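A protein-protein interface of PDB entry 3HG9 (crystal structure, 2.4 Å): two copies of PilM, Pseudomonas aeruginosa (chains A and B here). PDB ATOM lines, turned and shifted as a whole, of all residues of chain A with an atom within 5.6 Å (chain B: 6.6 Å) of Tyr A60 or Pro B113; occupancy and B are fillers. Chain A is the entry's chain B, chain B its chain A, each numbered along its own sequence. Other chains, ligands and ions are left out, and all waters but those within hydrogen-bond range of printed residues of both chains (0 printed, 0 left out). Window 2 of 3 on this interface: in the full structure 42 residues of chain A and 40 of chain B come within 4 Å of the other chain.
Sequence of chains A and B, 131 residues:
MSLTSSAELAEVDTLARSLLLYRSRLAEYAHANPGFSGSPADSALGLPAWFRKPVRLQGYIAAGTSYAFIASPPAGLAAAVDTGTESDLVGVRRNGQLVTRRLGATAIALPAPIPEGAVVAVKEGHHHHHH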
ATOM      1  N   LEU A  26     -22.100 -21.710 -18.823  1.00  0.00           N
ATOM      2  CA  LEU A  26     -23.534 -21.385 -18.879  1.00  0.00           C
ATOM      3  C   LEU A  26     -23.879 -20.501 -20.087  1.00  0.00           C
ATOM      4  O   LEU A  26     -24.816 -20.823 -20.791  1.00  0.00           O
ATOM      5  CB  LEU A  26     -23.984 -20.651 -17.638  1.00  0.00           C
ATOM      6  CG  LEU A  26     -23.885 -21.307 -16.277  1.00  0.00           C
ATOM      7  CD1 LEU A  26     -24.119 -20.179 -15.280  1.00  0.00           C
ATOM      8  CD2 LEU A  26     -24.949 -22.423 -16.134  1.00  0.00           C
ATOM      9  N   SER A  37     -34.353 -23.057 -17.574  1.00  0.00           N
ATOM     10  CA  SER A  37     -34.136 -22.237 -16.393  1.00  0.00           C
ATOM     11  C   SER A  37     -33.220 -22.848 -15.346  1.00  0.00           C
ATOM     12  O   SER A  37     -33.587 -23.137 -14.214  1.00  0.00           O
ATOM     13  CB  SER A  37     -35.445 -21.680 -15.835  1.00  0.00           C
ATOM     14  OG  SER A  37     -35.890 -20.629 -16.673  1.00  0.00           O
ATOM     15  N   GLY A  38     -31.960 -22.947 -15.757  1.00  0.00           N
ATOM     16  CA  GLY A  38     -30.911 -23.559 -14.961  1.00  0.00           C
ATOM     17  C   GLY A  38     -31.320 -24.948 -14.508  1.00  0.00           C
ATOM     18  O   GLY A  38     -32.239 -25.571 -15.035  1.00  0.00           O
ATOM     19  N   SER A  39     -30.642 -25.452 -13.506  1.00  0.00           N
ATOM     20  CA  SER A  39     -29.545 -24.804 -12.908  1.00  0.00           C
ATOM     21  C   SER A  39     -28.583 -25.906 -13.176  1.00  0.00           C
ATOM     22  O   SER A  39     -28.232 -26.623 -12.249  1.00  0.00           O
ATOM     23  CB  SER A  39     -29.777 -24.658 -11.413  1.00  0.00           C
ATOM     24  OG  SER A  39     -29.660 -23.296 -11.006  1.00  0.00           O
ATOM     25  N   PRO A  40     -28.134 -26.051 -14.445  1.00  0.00           N
ATOM     26  CA  PRO A  40     -27.575 -27.339 -14.868  1.00  0.00           C
ATOM     27  C   PRO A  40     -26.404 -27.853 -14.021  1.00  0.00           C
ATOM     28  O   PRO A  40     -25.590 -27.066 -13.576  1.00  0.00           O
ATOM     29  CB  PRO A  40     -27.135 -27.080 -16.337  1.00  0.00           C
ATOM     30  CG  PRO A  40     -26.943 -25.599 -16.462  1.00  0.00           C
ATOM     31  CD  PRO A  40     -27.754 -24.941 -15.362  1.00  0.00           C
ATOM     32  N   GLN A  58     -22.210 -21.106  -8.038  1.00  0.00           N
ATOM     33  CA  GLN A  58     -23.522 -21.520  -8.422  1.00  0.00           C
ATOM     34  C   GLN A  58     -23.815 -20.814  -9.680  1.00  0.00           C
ATOM     35  O   GLN A  58     -23.247 -19.776  -9.907  1.00  0.00           O
ATOM     36  CB  GLN A  58     -24.501 -21.145  -7.304  1.00  0.00           C
ATOM     37  CG  GLN A  58     -24.414 -22.122  -6.089  1.00  0.00           C
ATOM     38  CD  GLN A  58     -25.627 -21.992  -5.226  1.00  0.00           C
ATOM     39  OE1 GLN A  58     -25.556 -21.377  -4.137  1.00  0.00           O
ATOM     40  NE2 GLN A  58     -26.797 -22.449  -5.758  1.00  0.00           N
ATOM     41  N   GLY A  59     -24.674 -21.380 -10.509  1.00  0.00           N
ATOM     42  CA  GLY A  59     -25.082 -20.708 -11.706  1.00  0.00           C
ATOM     43  C   GLY A  59     -26.559 -20.920 -11.864  1.00  0.00           C
ATOM     44  O   GLY A  59     -27.063 -21.848 -11.261  1.00  0.00           O
ATOM     45  N   TYR A  60     -27.231 -20.083 -12.688  1.00  0.00           N
ATOM     46  CA  TYR A  60     -28.681 -20.156 -12.975  1.00  0.00           C
ATOM     47  C   TYR A  60     -28.921 -19.655 -14.417  1.00  0.00           C
ATOM     48  O   TYR A  60     -28.035 -19.069 -15.061  1.00  0.00           O
ATOM     49  CB  TYR A  60     -29.454 -19.275 -11.963  1.00  0.00           C
ATOM     50  CG  TYR A  60     -30.935 -19.582 -11.734  1.00  0.00           C
ATOM     51  CD1 TYR A  60     -31.333 -20.836 -11.250  1.00  0.00           C
ATOM     52  CD2 TYR A  60     -31.937 -18.616 -11.947  1.00  0.00           C
ATOM     53  CE1 TYR A  60     -32.690 -21.145 -11.029  1.00  0.00           C
ATOM     54  CE2 TYR A  60     -33.294 -18.914 -11.718  1.00  0.00           C
ATOM     55  CZ  TYR A  60     -33.658 -20.196 -11.251  1.00  0.00           C
ATOM     56  OH  TYR A  60     -34.962 -20.602 -11.002  1.00  0.00           O
ATOM     57  N   ILE A  61     -30.104 -19.861 -14.948  1.00  0.00           N
ATOM     58  CA  ILE A  61     -30.415 -19.213 -16.185  1.00  0.00           C
ATOM     59  C   ILE A  61     -31.805 -18.749 -15.887  1.00  0.00           C
ATOM     60  O   ILE A  61     -32.526 -19.334 -15.025  1.00  0.00           O
ATOM     61  CB  ILE A  61     -30.345 -20.163 -17.421  1.00  0.00           C
ATOM     62  CG1 ILE A  61     -28.903 -20.634 -17.620  1.00  0.00           C
ATOM     63  CG2 ILE A  61     -30.830 -19.465 -18.727  1.00  0.00           C
ATOM     64  CD1 ILE A  61     -28.712 -21.774 -18.572  1.00  0.00           C
ATOM     65  N   ALA A  62     -32.169 -17.676 -16.570  1.00  0.00           N
ATOM     66  CA  ALA A  62     -33.485 -17.106 -16.470  1.00  0.00           C
ATOM     67  C   ALA A  62     -33.597 -16.178 -17.707  1.00  0.00           C
ATOM     68  O   ALA A  62     -32.679 -15.388 -17.969  1.00  0.00           O
ATOM     69  CB  ALA A  62     -33.613 -16.345 -15.167  1.00  0.00           C
ATOM     70  N   THR A  65     -30.621 -15.737 -20.588  1.00  0.00           N
ATOM     71  CA  THR A  65     -29.516 -15.032 -19.969  1.00  0.00           C
ATOM     72  C   THR A  65     -29.062 -15.854 -18.770  1.00  0.00           C
ATOM     73  O   THR A  65     -29.918 -16.431 -18.051  1.00  0.00           O
ATOM     74  CB  THR A  65     -29.952 -13.734 -19.303  1.00  0.00           C
ATOM     75  OG1 THR A  65     -30.037 -13.961 -17.891  1.00  0.00           O
ATOM     76  CG2 THR A  65     -31.269 -13.176 -19.859  1.00  0.00           C
ATOM     77  N   SER A  66     -27.758 -15.867 -18.487  1.00  0.00           N
ATOM     78  CA  SER A  66     -27.317 -16.659 -17.349  1.00  0.00           C
ATOM     79  C   SER A  66     -26.536 -15.887 -16.281  1.00  0.00           C
ATOM     80  O   SER A  66     -25.917 -14.897 -16.565  1.00  0.00           O
ATOM     81  CB  SER A  66     -26.576 -17.918 -17.804  1.00  0.00           C
ATOM     82  OG  SER A  66     -25.887 -17.648 -18.995  1.00  0.00           O
ATOM     83  N   TYR A  67     -26.573 -16.393 -15.041  1.00  0.00           N
ATOM     84  CA  TYR A  67     -25.849 -15.819 -13.958  1.00  0.00           C
ATOM     85  C   TYR A  67     -24.948 -16.850 -13.282  1.00  0.00           C
ATOM     86  O   TYR A  67     -25.331 -18.011 -13.126  1.00  0.00           O
ATOM     87  CB  TYR A  67     -26.845 -15.355 -12.945  1.00  0.00           C
ATOM     88  CG  TYR A  67     -28.086 -14.749 -13.510  1.00  0.00           C
ATOM     89  CD1 TYR A  67     -28.450 -13.455 -13.168  1.00  0.00           C
ATOM     90  CD2 TYR A  67     -28.922 -15.457 -14.349  1.00  0.00           C
ATOM     91  CE1 TYR A  67     -29.642 -12.858 -13.652  1.00  0.00           C
ATOM     92  CE2 TYR A  67     -30.088 -14.871 -14.846  1.00  0.00           C
ATOM     93  CZ  TYR A  67     -30.453 -13.575 -14.489  1.00  0.00           C
ATOM     94  OH  TYR A  67     -31.636 -12.967 -14.999  1.00  0.00           O
ATOM     95  N   ALA A  68     -23.777 -16.434 -12.833  1.00  0.00           N
ATOM     96  CA  ALA A  68     -22.955 -17.318 -12.010  1.00  0.00           C
ATOM     97  C   ALA A  68     -22.706 -16.584 -10.704  1.00  0.00           C
ATOM     98  O   ALA A  68     -22.396 -15.390 -10.766  1.00  0.00           O
ATOM     99  CB  ALA A  68     -21.601 -17.609 -12.738  1.00  0.00           C
ATOM    100  N   PHE A  69     -22.874 -17.231  -9.545  1.00  0.00           N
ATOM    101  CA  PHE A  69     -22.795 -16.498  -8.290  1.00  0.00           C
ATOM    102  C   PHE A  69     -22.220 -17.244  -7.110  1.00  0.00           C
ATOM    103  O   PHE A  69     -22.524 -18.406  -6.884  1.00  0.00           O
ATOM    104  CB  PHE A  69     -24.166 -15.949  -7.885  1.00  0.00           C
ATOM    105  CG  PHE A  69     -25.277 -16.968  -7.880  1.00  0.00           C
ATOM    106  CD1 PHE A  69     -25.668 -17.594  -6.684  1.00  0.00           C
ATOM    107  CD2 PHE A  69     -25.972 -17.259  -9.073  1.00  0.00           C
ATOM    108  CE1 PHE A  69     -26.702 -18.516  -6.667  1.00  0.00           C
ATOM    109  CE2 PHE A  69     -27.016 -18.193  -9.094  1.00  0.00           C
ATOM    110  CZ  PHE A  69     -27.396 -18.841  -7.867  1.00  0.00           C
ATOM    111  N   ARG B  93     -25.973  -8.801  -4.857  1.00  0.00           N
ATOM    112  CA  ARG B  93     -27.430  -8.712  -4.594  1.00  0.00           C
ATOM    113  C   ARG B  93     -27.789  -7.825  -3.362  1.00  0.00           C
ATOM    114  O   ARG B  93     -27.555  -8.229  -2.194  1.00  0.00           O
ATOM    115  CB  ARG B  93     -28.038 -10.128  -4.511  1.00  0.00           C
ATOM    116  CG  ARG B  93     -29.433 -10.259  -3.952  1.00  0.00           C
ATOM    117  CD  ARG B  93     -30.515 -10.396  -4.996  1.00  0.00           C
ATOM    118  NE  ARG B  93     -31.051 -11.754  -5.078  1.00  0.00           N
ATOM    119  CZ  ARG B  93     -32.200 -12.107  -5.662  1.00  0.00           C
ATOM    120  NH1 ARG B  93     -32.524 -13.378  -5.685  1.00  0.00           N
ATOM    121  NH2 ARG B  93     -33.018 -11.216  -6.234  1.00  0.00           N
ATOM    122  N   LEU B 110     -33.793 -10.333 -10.383  1.00  0.00           N
ATOM    123  CA  LEU B 110     -32.804 -11.318  -9.938  1.00  0.00           C
ATOM    124  C   LEU B 110     -33.435 -12.681  -9.515  1.00  0.00           C
ATOM    125  O   LEU B 110     -33.955 -12.798  -8.427  1.00  0.00           O
ATOM    126  CB  LEU B 110     -31.853 -10.742  -8.889  1.00  0.00           C
ATOM    127  CG  LEU B 110     -30.669  -9.945  -9.463  1.00  0.00           C
ATOM    128  CD1 LEU B 110     -29.552  -9.716  -8.419  1.00  0.00           C
ATOM    129  CD2 LEU B 110     -30.156 -10.542 -10.777  1.00  0.00           C
ATOM    130  N   PRO B 111     -33.357 -13.712 -10.388  1.00  0.00           N
ATOM    131  CA  PRO B 111     -33.991 -14.985 -10.170  1.00  0.00           C
ATOM    132  C   PRO B 111     -34.058 -15.352  -8.678  1.00  0.00           C
ATOM    133  O   PRO B 111     -33.230 -14.905  -7.881  1.00  0.00           O
ATOM    134  CB  PRO B 111     -33.026 -15.950 -10.850  1.00  0.00           C
ATOM    135  CG  PRO B 111     -32.450 -15.207 -11.966  1.00  0.00           C
ATOM    136  CD  PRO B 111     -32.362 -13.794 -11.484  1.00  0.00           C
ATOM    137  N   ALA B 112     -35.034 -16.172  -8.335  1.00  0.00           N
ATOM    138  CA  ALA B 112     -35.282 -16.619  -6.960  1.00  0.00           C
ATOM    139  C   ALA B 112     -34.040 -17.031  -6.068  1.00  0.00           C
ATOM    140  O   ALA B 112     -33.920 -16.548  -4.922  1.00  0.00           O
ATOM    141  CB  ALA B 112     -36.340 -17.695  -6.994  1.00  0.00           C
ATOM    142  N   PRO B 113     -33.122 -17.891  -6.584  1.00  0.00           N
ATOM    143  CA  PRO B 113     -31.999 -18.482  -5.851  1.00  0.00           C
ATOM    144  C   PRO B 113     -30.754 -17.667  -5.488  1.00  0.00           C
ATOM    145  O   PRO B 113     -29.874 -18.195  -4.740  1.00  0.00           O
ATOM    146  CB  PRO B 113     -31.559 -19.618  -6.770  1.00  0.00           C
ATOM    147  CG  PRO B 113     -32.781 -20.001  -7.454  1.00  0.00           C
ATOM    148  CD  PRO B 113     -33.374 -18.668  -7.802  1.00  0.00           C
ATOM    149  N   ILE B 114     -30.610 -16.460  -6.021  1.00  0.00           N
ATOM    150  CA  ILE B 114     -29.431 -15.726  -5.673  1.00  0.00           C
ATOM    151  C   ILE B 114     -29.620 -15.014  -4.357  1.00  0.00           C
ATOM    152  O   ILE B 114     -30.474 -14.138  -4.223  1.00  0.00           O
ATOM    153  CB  ILE B 114     -28.757 -14.862  -6.835  1.00  0.00           C
ATOM    154  CG1 ILE B 114     -28.138 -13.583  -6.270  1.00  0.00           C
ATOM    155  CG2 ILE B 114     -29.662 -14.625  -8.059  1.00  0.00           C
ATOM    156  CD1 ILE B 114     -26.771 -13.795  -5.682  1.00  0.00           C
ATOM    157  N   PRO B 115     -28.849 -15.420  -3.343  1.00  0.00           N
ATOM    158  CA  PRO B 115     -29.141 -14.766  -2.081  1.00  0.00           C
ATOM    159  C   PRO B 115     -28.749 -13.314  -2.068  1.00  0.00           C
ATOM    160  O   PRO B 115     -27.827 -12.905  -2.779  1.00  0.00           O
ATOM    161  CB  PRO B 115     -28.285 -15.555  -1.081  1.00  0.00           C
ATOM    162  CG  PRO B 115     -27.329 -16.228  -1.855  1.00  0.00           C
ATOM    163  CD  PRO B 115     -28.008 -16.600  -3.127  1.00  0.00           C
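The backbone carbonyl oxygen of Leu B110 sits at hydrogen-bond distance from the guanidinium group of Arg B93 (2.9 Å).
O of Pro B111 sits at hydrogen-bond distance from NH1 of Arg B93 (2.8 Å).
O of Gln A58 is in hydrogen-bond range of N of Phe A69 (2.6 Å).
O of Tyr A67 lies within hydrogen-bond range of N of Tyr A60 (2.8 Å).
The side-chain hydroxyl of Tyr A67 sits close to the side-chain hydroxyl of Thr A65 (3.5 Å).
OG1 of Thr A65 sits at hydrogen-bond distance from O of Ala A62 (3.0 Å).
Tyr A60 touches Pro B111.
CG of Pro B113 touches CE1 of Tyr A60, 3.8 Å away.
Pro B111 touches Ala A62.
Tyr A67 touches Leu B110 (CE1 to CD2, 3.7 Å).
Pro B111 touches Tyr A67 (CD to CZ, 3.6 Å).
Phe A69 touches Pro B113 (CE1 to O, 3.7 Å).
Pro B113 touches just these residues of chain A: Tyr A60 and Phe A69.
Of the printed residues of chain A, Leu B110 touches Tyr A67 (3.7 Å).
Of the printed residues of chain B, Ala A62 touches Pro B111.
Printed residues of chain B within 4 Å of Tyr A67: Leu B110 (3.7 Å) and Pro B111 (3.6 Å).
Of the printed residues of chain B, Phe A69 touches Pro B113.
The nearest residue of chain B that does not touch Tyr A60 is Ala B112 (4.7 Å).
The nearest printed residue of chain A that does not touch Pro B111 is Ile A61 (5.1 Å).
Printed residues of chain B that touch a printed residue of chain A: Leu B110, Pro B111 and Pro B113.
Printed residues of chain A that touch a printed residue of chain B: Tyr A60, Ala A62, Tyr A67 and Phe A69.
Hydrophobic or aromatic side chains of chain A within 4 Å of the printed part of chain B: Tyr A60, Ala A62, Tyr A67 and Phe A69.
No position is printed for both chains.
Of the 6 pairs that touch across the chains among the printed residues, none has its exchanged pair printed and touching as well.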
